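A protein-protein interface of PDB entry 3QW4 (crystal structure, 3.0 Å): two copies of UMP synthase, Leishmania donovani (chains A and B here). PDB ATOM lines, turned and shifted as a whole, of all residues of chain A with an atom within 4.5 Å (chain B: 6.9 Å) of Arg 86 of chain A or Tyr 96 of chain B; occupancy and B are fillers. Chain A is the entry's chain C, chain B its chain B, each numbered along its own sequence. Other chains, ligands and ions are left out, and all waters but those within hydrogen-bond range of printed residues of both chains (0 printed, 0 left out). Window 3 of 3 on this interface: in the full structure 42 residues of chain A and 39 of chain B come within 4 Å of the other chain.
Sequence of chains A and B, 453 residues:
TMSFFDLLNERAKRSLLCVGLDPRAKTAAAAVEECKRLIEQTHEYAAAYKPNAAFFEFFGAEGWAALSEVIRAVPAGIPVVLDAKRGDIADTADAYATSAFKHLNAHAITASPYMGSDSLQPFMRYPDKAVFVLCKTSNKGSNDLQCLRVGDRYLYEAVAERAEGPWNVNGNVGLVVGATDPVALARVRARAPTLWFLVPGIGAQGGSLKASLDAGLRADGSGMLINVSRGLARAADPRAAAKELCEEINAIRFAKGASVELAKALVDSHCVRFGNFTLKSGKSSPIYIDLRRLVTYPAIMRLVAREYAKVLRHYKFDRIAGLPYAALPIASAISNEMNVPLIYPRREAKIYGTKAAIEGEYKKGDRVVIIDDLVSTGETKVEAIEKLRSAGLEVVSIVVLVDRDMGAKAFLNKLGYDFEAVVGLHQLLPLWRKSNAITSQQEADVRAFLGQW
The guanidinium group (NH1) of Arg 86 of chain A sits close to the guanidinium group (NH1) of Arg 86 of chain B (2.9 Å).
The guanidinium group (NH2) of Arg 86 of chain B lies within salt-bridge range of the side-chain carboxylate (OE1) of Glu 57 of chain A (2.6 Å).
The side-chain carboxylate of Glu 57 of chain B is in salt-bridge range of the guanidinium group of Arg 86 of chain A (2.7 Å).
The backbone NH of Ser 112 of chain A is in hydrogen-bond range of the backbone carbonyl oxygen of Arg 86 of chain A, 2.9 Å away.
The side-chain hydroxyl of Thr 110 of chain A sits at hydrogen-bond distance from the backbone NH of Ala 84 of chain A, at 2.9 Å.
The guanidinium group (NH1) of Arg 86 of chain B sits at hydrogen-bond distance from the backbone carbonyl oxygen (O) of Ala 84 of chain B, 3.1 Å away.
N of Arg 86 of chain A sits at hydrogen-bond distance from O of Thr 110 of chain A, 3.0 Å away.
The side-chain carboxylate of Glu 57 of chain B lies within salt-bridge range of the guanidinium group of Arg 86 of chain B (3.97 Å).
The backbone carbonyl oxygen (O) of Ala 84 of chain A lies within hydrogen-bond range of the guanidinium group (NH1) of Arg 86 of chain A (3.1 Å).
Among the printed residues, pairs that only touch across the chains: Gly 87 of chain A with Lys 85 of chain B, Glu 57 of chain A with Tyr 96 of chain B, Tyr 96 of chain A with Glu 57 of chain B, Ala 54 of chain A with Tyr 96 of chain B, Ala 54 of chain A with Thr 92 of chain B, Ala 53 of chain A with Tyr 96 of chain B, Glu 57 of chain A with Ser 99 of chain B, Arg 86 of chain A with Tyr 96 of chain B and Ala 84 of chain A with Tyr 96 of chain B.
Of the printed residues of chain B, Ala 54 of chain A touches Thr 92 (3.7 Å) and Tyr 96 (3.6 Å).
Of the printed residues of chain B, Glu 57 of chain A touches Arg 86 (2.6 Å), Tyr 96 (3.4 Å) and Ser 99 (3.8 Å).
Of the printed residues of chain B, Ala 84 of chain A touches Tyr 96 (3.96 Å).
Of chain B, only Glu 57 (2.7 Å), Arg 86 (2.9 Å) and Tyr 96 (3.96 Å) come within 4 Å of Arg 86 of chain A.
Printed residues of chain B within 4 Å of Tyr 96 of chain A: Glu 57.
Printed residues of chain A within 4 Å of Thr 92 of chain B: Ala 54.
Of chain A, only Ala 53 (3.7 Å), Ala 54 (3.6 Å), Glu 57 (3.4 Å), Ala 84 (3.96 Å) and Arg 86 (3.96 Å) come within 4 Å of Tyr 96 of chain B.
Phe 101 of chain B touches none of the printed residues of chain A.
Phe 123 of chain B touches none of the printed residues of chain A.
The nearest printed residue of chain B that does not touch Ala 54 of chain A is Ala 95 of chain B (4.1 Å).
Hydrophobic or aromatic side chains of chain B that line the printed part of chain A: Tyr 96.
Printed residues of chain A that touch a printed residue of chain B: Ala 53, Ala 54, Glu 57, Ala 84, Arg 86, Gly 87 and Tyr 96.
Hydrophobic or aromatic side chains of chain A that line the printed part of chain B: Ala 53, Ala 54 and Tyr 96.
Glu 57 of chain A touches Arg 86 of chain B, and with the chains exchanged Arg 86 of chain A touches Glu 57 of chain B.
Ala 84 of chain A touches Tyr 96 of chain B, but with the chains exchanged Tyr 96 of chain A does not touch Ala 84 of chain B (4.1 Å).
Arg 86 of chain A touches Tyr 96 of chain B, but with the chains exchanged Tyr 96 of chain A does not touch Arg 86 of chain B (4.2 Å).
Gly 87 of chain A touches Lys 85 of chain B, but with the chains exchanged Lys 85 of chain A does not touch Gly 87 of chain B (4.1 Å).
Positions printed for both chains: 57, 84, 85, 86, 87, 96, 109 and 123.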
ATOM      1  N   ALA A  53      18.283 -26.431  16.972  1.00  0.00           N
ATOM      2  CA  ALA A  53      17.222 -26.422  17.990  1.00  0.00           C
ATOM      3  C   ALA A  53      15.991 -25.622  17.600  1.00  0.00           C
ATOM      4  O   ALA A  53      14.870 -26.020  17.910  1.00  0.00           O
ATOM      5  CB  ALA A  53      17.766 -25.936  19.327  1.00  0.00           C
ATOM      6  N   ALA A  54      16.215 -24.514  16.900  1.00  0.00           N
ATOM      7  CA  ALA A  54      15.163 -23.556  16.571  1.00  0.00           C
ATOM      8  C   ALA A  54      13.894 -24.177  15.992  1.00  0.00           C
ATOM      9  O   ALA A  54      12.785 -23.880  16.438  1.00  0.00           O
ATOM     10  CB  ALA A  54      15.706 -22.486  15.641  1.00  0.00           C
ATOM     11  N   GLU A  57      12.237 -26.417  18.637  1.00  0.00           N
ATOM     12  CA  GLU A  57      11.716 -25.578  19.701  1.00  0.00           C
ATOM     13  C   GLU A  57      10.489 -24.815  19.222  1.00  0.00           C
ATOM     14  O   GLU A  57       9.703 -24.311  20.023  1.00  0.00           O
ATOM     15  CB  GLU A  57      12.799 -24.601  20.126  1.00  0.00           C
ATOM     16  CG  GLU A  57      12.685 -24.139  21.549  1.00  0.00           C
ATOM     17  CD  GLU A  57      13.777 -23.166  21.932  1.00  0.00           C
ATOM     18  OE1 GLU A  57      13.435 -22.172  22.612  1.00  0.00           O
ATOM     19  OE2 GLU A  57      14.961 -23.383  21.558  1.00  0.00           O
ATOM     20  N   ALA A  84      22.648 -25.031  18.878  1.00  0.00           N
ATOM     21  CA  ALA A  84      21.842 -24.383  19.892  1.00  0.00           C
ATOM     22  C   ALA A  84      22.387 -22.993  20.182  1.00  0.00           C
ATOM     23  O   ALA A  84      21.667 -22.132  20.684  1.00  0.00           O
ATOM     24  CB  ALA A  84      21.845 -25.215  21.143  1.00  0.00           C
ATOM     25  N   LYS A  85      23.664 -22.788  19.856  1.00  0.00           N
ATOM     26  CA  LYS A  85      24.361 -21.509  20.034  1.00  0.00           C
ATOM     27  C   LYS A  85      24.214 -20.946  21.454  1.00  0.00           C
ATOM     28  O   LYS A  85      23.825 -19.802  21.643  1.00  0.00           O
ATOM     29  CB  LYS A  85      23.932 -20.492  18.960  1.00  0.00           C
ATOM     30  N   ARG A  86      24.531 -21.765  22.451  1.00  0.00           N
ATOM     31  CA  ARG A  86      24.375 -21.373  23.848  1.00  0.00           C
ATOM     32  C   ARG A  86      25.507 -20.467  24.304  1.00  0.00           C
ATOM     33  O   ARG A  86      26.456 -20.232  23.566  1.00  0.00           O
ATOM     34  CB  ARG A  86      24.272 -22.610  24.748  1.00  0.00           C
ATOM     35  CG  ARG A  86      23.126 -23.578  24.396  1.00  0.00           C
ATOM     36  CD  ARG A  86      21.765 -22.888  24.307  1.00  0.00           C
ATOM     37  NE  ARG A  86      20.663 -23.832  24.122  1.00  0.00           N
ATOM     38  CZ  ARG A  86      19.556 -23.571  23.425  1.00  0.00           C
ATOM     39  NH1 ARG A  86      19.398 -22.402  22.819  1.00  0.00           N
ATOM     40  NH2 ARG A  86      18.604 -24.484  23.309  1.00  0.00           N
ATOM     41  N   GLY A  87      25.391 -19.943  25.521  1.00  0.00           N
ATOM     42  CA  GLY A  87      26.403 -19.060  26.089  1.00  0.00           C
ATOM     43  C   GLY A  87      25.789 -18.156  27.131  1.00  0.00           C
ATOM     44  O   GLY A  87      25.097 -17.203  26.790  1.00  0.00           O
ATOM     45  N   TYR A  96      22.422 -25.818  30.669  1.00  0.00           N
ATOM     46  CA  TYR A  96      22.400 -26.001  29.231  1.00  0.00           C
ATOM     47  C   TYR A  96      23.305 -27.155  28.805  1.00  0.00           C
ATOM     48  O   TYR A  96      23.015 -27.849  27.832  1.00  0.00           O
ATOM     49  CB  TYR A  96      22.829 -24.715  28.523  1.00  0.00           C
ATOM     50  CG  TYR A  96      21.720 -23.733  28.191  1.00  0.00           C
ATOM     51  CD1 TYR A  96      21.888 -22.364  28.435  1.00  0.00           C
ATOM     52  CD2 TYR A  96      20.519 -24.160  27.613  1.00  0.00           C
ATOM     53  CE1 TYR A  96      20.889 -21.446  28.124  1.00  0.00           C
ATOM     54  CE2 TYR A  96      19.507 -23.250  27.299  1.00  0.00           C
ATOM     55  CZ  TYR A  96      19.699 -21.894  27.559  1.00  0.00           C
ATOM     56  OH  TYR A  96      18.709 -20.986  27.246  1.00  0.00           O
ATOM     57  N   ILE A 109      28.078 -29.148  20.672  1.00  0.00           N
ATOM     58  CA  ILE A 109      27.188 -27.987  20.704  1.00  0.00           C
ATOM     59  C   ILE A 109      27.849 -26.739  20.119  1.00  0.00           C
ATOM     60  O   ILE A 109      29.061 -26.554  20.253  1.00  0.00           O
ATOM     61  CB  ILE A 109      26.725 -27.691  22.143  1.00  0.00           C
ATOM     62  CG1 ILE A 109      25.570 -26.695  22.143  1.00  0.00           C
ATOM     63  CG2 ILE A 109      27.892 -27.215  23.003  1.00  0.00           C
ATOM     64  CD1 ILE A 109      24.741 -26.727  23.387  1.00  0.00           C
ATOM     65  N   THR A 110      27.049 -25.897  19.466  1.00  0.00           N
ATOM     66  CA  THR A 110      27.492 -24.555  19.066  1.00  0.00           C
ATOM     67  C   THR A 110      27.322 -23.558  20.220  1.00  0.00           C
ATOM     68  O   THR A 110      26.400 -23.687  21.025  1.00  0.00           O
ATOM     69  CB  THR A 110      26.734 -24.031  17.827  1.00  0.00           C
ATOM     70  OG1 THR A 110      25.324 -24.109  18.055  1.00  0.00           O
ATOM     71  CG2 THR A 110      27.092 -24.835  16.590  1.00  0.00           C
ATOM     72  N   ALA A 111      28.215 -22.571  20.293  1.00  0.00           N
ATOM     73  CA  ALA A 111      28.222 -21.586  21.381  1.00  0.00           C
ATOM     74  C   ALA A 111      28.792 -20.210  20.983  1.00  0.00           C
ATOM     75  O   ALA A 111      29.549 -20.093  20.018  1.00  0.00           O
ATOM     76  CB  ALA A 111      28.962 -22.148  22.593  1.00  0.00           C
ATOM     77  N   SER A 112      28.418 -19.171  21.730  1.00  0.00           N
ATOM     78  CA  SER A 112      28.886 -17.807  21.463  1.00  0.00           C
ATOM     79  C   SER A 112      30.124 -17.482  22.276  1.00  0.00           C
ATOM     80  O   SER A 112      30.169 -17.763  23.475  1.00  0.00           O
ATOM     81  CB  SER A 112      27.792 -16.776  21.756  1.00  0.00           C
ATOM     82  OG  SER A 112      28.342 -15.506  22.095  1.00  0.00           O
ATOM     83  N   PHE A 123      30.849 -26.157  29.192  1.00  0.00           N
ATOM     84  CA  PHE A 123      30.672 -27.038  28.040  1.00  0.00           C
ATOM     85  C   PHE A 123      31.961 -27.759  27.661  1.00  0.00           C
ATOM     86  O   PHE A 123      31.935 -28.923  27.274  1.00  0.00           O
ATOM     87  CB  PHE A 123      30.175 -26.247  26.832  1.00  0.00           C
ATOM     88  CG  PHE A 123      28.842 -25.596  27.034  1.00  0.00           C
ATOM     89  CD1 PHE A 123      27.664 -26.334  26.936  1.00  0.00           C
ATOM     90  CD2 PHE A 123      28.758 -24.235  27.298  1.00  0.00           C
ATOM     91  CE1 PHE A 123      26.421 -25.730  27.110  1.00  0.00           C
ATOM     92  CE2 PHE A 123      27.516 -23.618  27.475  1.00  0.00           C
ATOM     93  CZ  PHE A 123      26.345 -24.373  27.381  1.00  0.00           C
ATOM     94  N   GLU B  57      14.335 -25.519  30.322  1.00  0.00           N
ATOM     95  CA  GLU B  57      14.783 -26.404  29.249  1.00  0.00           C
ATOM     96  C   GLU B  57      15.433 -27.656  29.833  1.00  0.00           C
ATOM     97  O   GLU B  57      15.509 -28.690  29.168  1.00  0.00           O
ATOM     98  CB  GLU B  57      15.773 -25.667  28.353  1.00  0.00           C
ATOM     99  CG  GLU B  57      15.363 -25.606  26.907  1.00  0.00           C
ATOM    100  CD  GLU B  57      16.320 -24.751  26.071  1.00  0.00           C
ATOM    101  OE1 GLU B  57      17.332 -25.321  25.586  1.00  0.00           O
ATOM    102  OE2 GLU B  57      16.082 -23.516  25.916  1.00  0.00           O
ATOM    103  N   LEU B  82      12.111 -12.545  28.329  1.00  0.00           N
ATOM    104  CA  LEU B  82      12.609 -13.902  28.174  1.00  0.00           C
ATOM    105  C   LEU B  82      14.117 -13.876  27.981  1.00  0.00           C
ATOM    106  O   LEU B  82      14.615 -13.265  27.029  1.00  0.00           O
ATOM    107  CB  LEU B  82      11.932 -14.609  27.006  1.00  0.00           C
ATOM    108  CG  LEU B  82      12.366 -16.063  26.804  1.00  0.00           C
ATOM    109  CD1 LEU B  82      11.807 -16.941  27.894  1.00  0.00           C
ATOM    110  CD2 LEU B  82      11.986 -16.602  25.432  1.00  0.00           C
ATOM    111  N   ALA B  84      16.923 -15.726  26.850  1.00  0.00           N
ATOM    112  CA  ALA B  84      17.157 -16.902  26.027  1.00  0.00           C
ATOM    113  C   ALA B  84      18.440 -16.758  25.223  1.00  0.00           C
ATOM    114  O   ALA B  84      18.978 -17.746  24.702  1.00  0.00           O
ATOM    115  CB  ALA B  84      15.965 -17.142  25.103  1.00  0.00           C
ATOM    116  N   LYS B  85      18.924 -15.526  25.128  1.00  0.00           N
ATOM    117  CA  LYS B  85      20.130 -15.216  24.365  1.00  0.00           C
ATOM    118  C   LYS B  85      20.117 -15.833  22.971  1.00  0.00           C
ATOM    119  O   LYS B  85      20.926 -16.703  22.658  1.00  0.00           O
ATOM    120  CB  LYS B  85      21.378 -15.631  25.138  1.00  0.00           C
ATOM    121  CG  LYS B  85      21.616 -14.757  26.335  1.00  0.00           C
ATOM    122  CD  LYS B  85      22.534 -15.396  27.334  1.00  0.00           C
ATOM    123  CE  LYS B  85      22.438 -14.640  28.639  1.00  0.00           C
ATOM    124  NZ  LYS B  85      21.205 -15.020  29.379  1.00  0.00           N
ATOM    125  N   ARG B  86      19.184 -15.369  22.145  1.00  0.00           N
ATOM    126  CA  ARG B  86      19.063 -15.848  20.782  1.00  0.00           C
ATOM    127  C   ARG B  86      19.998 -15.113  19.816  1.00  0.00           C
ATOM    128  O   ARG B  86      20.506 -14.024  20.111  1.00  0.00           O
ATOM    129  CB  ARG B  86      17.610 -15.802  20.296  1.00  0.00           C
ATOM    130  CG  ARG B  86      16.639 -16.719  21.046  1.00  0.00           C
ATOM    131  CD  ARG B  86      17.137 -18.152  21.223  1.00  0.00           C
ATOM    132  NE  ARG B  86      16.117 -18.989  21.856  1.00  0.00           N
ATOM    133  CZ  ARG B  86      16.359 -19.909  22.793  1.00  0.00           C
ATOM    134  NH1 ARG B  86      17.597 -20.121  23.237  1.00  0.00           N
ATOM    135  NH2 ARG B  86      15.356 -20.602  23.312  1.00  0.00           N
ATOM    136  N   GLY B  87      20.229 -15.751  18.666  1.00  0.00           N
ATOM    137  CA  GLY B  87      21.110 -15.223  17.636  1.00  0.00           C
ATOM    138  C   GLY B  87      21.571 -16.330  16.717  1.00  0.00           C
ATOM    139  O   GLY B  87      22.307 -17.240  17.134  1.00  0.00           O
ATOM    140  N   ASP B  88      21.094 -16.251  15.474  1.00  0.00           N
ATOM    141  CA  ASP B  88      21.538 -17.096  14.372  1.00  0.00           C
ATOM    142  C   ASP B  88      21.296 -16.352  13.059  1.00  0.00           C
ATOM    143  O   ASP B  88      21.041 -15.148  13.069  1.00  0.00           O
ATOM    144  CB  ASP B  88      20.816 -18.443  14.386  1.00  0.00           C
ATOM    145  CG  ASP B  88      21.755 -19.606  14.070  1.00  0.00           C
ATOM    146  OD1 ASP B  88      22.233 -19.718  12.900  1.00  0.00           O
ATOM    147  OD2 ASP B  88      22.011 -20.407  15.010  1.00  0.00           O
ATOM    148  N   ASP B  91      16.984 -16.495   8.687  1.00  0.00           N
ATOM    149  CA  ASP B  91      15.980 -17.532   8.420  1.00  0.00           C
ATOM    150  C   ASP B  91      15.694 -18.394   9.647  1.00  0.00           C
ATOM    151  O   ASP B  91      14.536 -18.741   9.923  1.00  0.00           O
ATOM    152  CB  ASP B  91      16.411 -18.421   7.246  1.00  0.00           C
ATOM    153  CG  ASP B  91      16.433 -17.674   5.912  1.00  0.00           C
ATOM    154  OD1 ASP B  91      15.528 -16.839   5.660  1.00  0.00           O
ATOM    155  OD2 ASP B  91      17.358 -17.936   5.107  1.00  0.00           O
ATOM    156  N   THR B  92      16.757 -18.732  10.374  1.00  0.00           N
ATOM    157  CA  THR B  92      16.657 -19.490  11.620  1.00  0.00           C
ATOM    158  C   THR B  92      16.106 -18.607  12.744  1.00  0.00           C
ATOM    159  O   THR B  92      15.269 -19.039  13.541  1.00  0.00           O
ATOM    160  CB  THR B  92      18.038 -20.059  12.021  1.00  0.00           C
ATOM    161  OG1 THR B  92      18.478 -20.982  11.022  1.00  0.00           O
ATOM    162  CG2 THR B  92      17.982 -20.776  13.350  1.00  0.00           C
ATOM    163  N   ALA B  93      16.573 -17.364  12.791  1.00  0.00           N
ATOM    164  CA  ALA B  93      16.190 -16.441  13.840  1.00  0.00           C
ATOM    165  C   ALA B  93      14.681 -16.191  13.905  1.00  0.00           C
ATOM    166  O   ALA B  93      14.149 -15.888  14.973  1.00  0.00           O
ATOM    167  CB  ALA B  93      16.950 -15.140  13.693  1.00  0.00           C
ATOM    168  N   ASP B  94      14.004 -16.318  12.762  1.00  0.00           N
ATOM    169  CA  ASP B  94      12.548 -16.138  12.667  1.00  0.00           C
ATOM    170  C   ASP B  94      11.823 -17.140  13.543  1.00  0.00           C
ATOM    171  O   ASP B  94      10.924 -16.789  14.309  1.00  0.00           O
ATOM    172  CB  ASP B  94      12.074 -16.288  11.219  1.00  0.00           C
ATOM    173  CG  ASP B  94      12.565 -15.168  10.316  1.00  0.00           C
ATOM    174  OD1 ASP B  94      12.882 -14.065  10.815  1.00  0.00           O
ATOM    175  OD2 ASP B  94      12.624 -15.389   9.089  1.00  0.00           O
ATOM    176  N   ALA B  95      12.238 -18.395  13.427  1.00  0.00           N
ATOM    177  CA  ALA B  95      11.709 -19.464  14.252  1.00  0.00           C
ATOM    178  C   ALA B  95      11.917 -19.200  15.757  1.00  0.00           C
ATOM    179  O   ALA B  95      11.100 -19.616  16.580  1.00  0.00           O
ATOM    180  CB  ALA B  95      12.330 -20.796  13.838  1.00  0.00           C
ATOM    181  N   TYR B  96      13.009 -18.514  16.103  1.00  0.00           N
ATOM    182  CA  TYR B  96      13.293 -18.168  17.488  1.00  0.00           C
ATOM    183  C   TYR B  96      12.441 -17.006  17.955  1.00  0.00           C
ATOM    184  O   TYR B  96      11.963 -17.001  19.090  1.00  0.00           O
ATOM    185  CB  TYR B  96      14.766 -17.836  17.672  1.00  0.00           C
ATOM    186  CG  TYR B  96      15.637 -19.019  18.047  1.00  0.00           C
ATOM    187  CD1 TYR B  96      16.967 -19.094  17.620  1.00  0.00           C
ATOM    188  CD2 TYR B  96      15.136 -20.058  18.844  1.00  0.00           C
ATOM    189  CE1 TYR B  96      17.772 -20.170  17.974  1.00  0.00           C
ATOM    190  CE2 TYR B  96      15.935 -21.140  19.206  1.00  0.00           C
ATOM    191  CZ  TYR B  96      17.247 -21.190  18.762  1.00  0.00           C
ATOM    192  OH  TYR B  96      18.033 -22.265  19.107  1.00  0.00           O
ATOM    193  N   ALA B  97      12.249 -16.033  17.066  1.00  0.00           N
ATOM    194  CA  ALA B  97      11.439 -14.846  17.354  1.00  0.00           C
ATOM    195  C   ALA B  97       9.947 -15.181  17.430  1.00  0.00           C
ATOM    196  O   ALA B  97       9.240 -14.681  18.308  1.00  0.00           O
ATOM    197  CB  ALA B  97      11.705 -13.747  16.328  1.00  0.00           C
ATOM    198  N   THR B  98       9.467 -16.030  16.526  1.00  0.00           N
ATOM    199  CA  THR B  98       8.086 -16.480  16.616  1.00  0.00           C
ATOM    200  C   THR B  98       7.874 -17.204  17.939  1.00  0.00           C
ATOM    201  O   THR B  98       6.946 -16.884  18.677  1.00  0.00           O
ATOM    202  CB  THR B  98       7.690 -17.389  15.428  1.00  0.00           C
ATOM    203  OG1 THR B  98       7.943 -16.701  14.199  1.00  0.00           O
ATOM    204  CG2 THR B  98       6.207 -17.768  15.480  1.00  0.00           C
ATOM    205  N   SER B  99       8.754 -18.161  18.235  1.00  0.00           N
ATOM    206  CA  SER B  99       8.644 -18.996  19.416  1.00  0.00           C
ATOM    207  C   SER B  99       8.507 -18.159  20.677  1.00  0.00           C
ATOM    208  O   SER B  99       7.662 -18.434  21.525  1.00  0.00           O
ATOM    209  CB  SER B  99       9.866 -19.897  19.521  1.00  0.00           C
ATOM    210  OG  SER B  99       9.876 -20.624  20.741  1.00  0.00           O
ATOM    211  N   ALA B 100       9.344 -17.129  20.786  1.00  0.00           N
ATOM    212  CA  ALA B 100       9.351 -16.240  21.942  1.00  0.00           C
ATOM    213  C   ALA B 100       8.125 -15.329  21.995  1.00  0.00           C
ATOM    214  O   ALA B 100       7.424 -15.291  22.999  1.00  0.00           O
ATOM    215  CB  ALA B 100      10.625 -15.420  21.967  1.00  0.00           C
ATOM    216  N   PHE B 101       7.851 -14.615  20.908  1.00  0.00           N
ATOM    217  CA  PHE B 101       6.817 -13.579  20.918  1.00  0.00           C
ATOM    218  C   PHE B 101       5.393 -14.072  20.692  1.00  0.00           C
ATOM    219  O   PHE B 101       4.451 -13.521  21.258  1.00  0.00           O
ATOM    220  CB  PHE B 101       7.152 -12.466  19.921  1.00  0.00           C
ATOM    221  CG  PHE B 101       8.496 -11.817  20.156  1.00  0.00           C
ATOM    222  CD1 PHE B 101       8.946 -11.540  21.441  1.00  0.00           C
ATOM    223  CD2 PHE B 101       9.308 -11.472  19.083  1.00  0.00           C
ATOM    224  CE1 PHE B 101      10.184 -10.943  21.644  1.00  0.00           C
ATOM    225  CE2 PHE B 101      10.556 -10.866  19.283  1.00  0.00           C
ATOM    226  CZ  PHE B 101      10.990 -10.603  20.558  1.00  0.00           C
ATOM    227  N   LEU B 104       5.206 -18.332  23.114  1.00  0.00           N
ATOM    228  CA  LEU B 104       5.403 -18.146  24.536  1.00  0.00           C
ATOM    229  C   LEU B 104       4.786 -16.845  25.051  1.00  0.00           C
ATOM    230  O   LEU B 104       4.542 -16.709  26.257  1.00  0.00           O
ATOM    231  CB  LEU B 104       6.893 -18.187  24.848  1.00  0.00           C
ATOM    232  CG  LEU B 104       7.591 -19.543  24.730  1.00  0.00           C
ATOM    233  CD1 LEU B 104       9.105 -19.348  24.634  1.00  0.00           C
ATOM    234  CD2 LEU B 104       7.215 -20.452  25.900  1.00  0.00           C
ATOM    235  N   ILE B 109      13.119 -10.044  24.665  1.00  0.00           N
ATOM    236  CA  ILE B 109      14.057 -11.141  24.654  1.00  0.00           C
ATOM    237  C   ILE B 109      15.483 -10.606  24.774  1.00  0.00           C
ATOM    238  O   ILE B 109      15.777  -9.469  24.369  1.00  0.00           O
ATOM    239  CB  ILE B 109      13.885 -12.014  23.372  1.00  0.00           C
ATOM    240  CG1 ILE B 109      14.622 -13.353  23.509  1.00  0.00           C
ATOM    241  CG2 ILE B 109      14.325 -11.266  22.104  1.00  0.00           C
ATOM    242  CD1 ILE B 109      14.192 -14.398  22.493  1.00  0.00           C
ATOM    243  N   PHE B 123      14.165 -10.181  15.374  1.00  0.00           N
ATOM    244  CA  PHE B 123      13.596  -9.921  16.690  1.00  0.00           C
ATOM    245  C   PHE B 123      13.082  -8.496  16.718  1.00  0.00           C
ATOM    246  O   PHE B 123      11.957  -8.228  17.136  1.00  0.00           O
ATOM    247  CB  PHE B 123      14.638 -10.132  17.794  1.00  0.00           C
ATOM    248  CG  PHE B 123      15.140 -11.528  17.889  1.00  0.00           C
ATOM    249  CD1 PHE B 123      14.411 -12.499  18.555  1.00  0.00           C
ATOM    250  CD2 PHE B 123      16.342 -11.884  17.304  1.00  0.00           C
ATOM    251  CE1 PHE B 123      14.875 -13.821  18.637  1.00  0.00           C
ATOM    252  CE2 PHE B 123      16.819 -13.202  17.375  1.00  0.00           C
ATOM    253  CZ  PHE B 123      16.081 -14.168  18.044  1.00  0.00           C
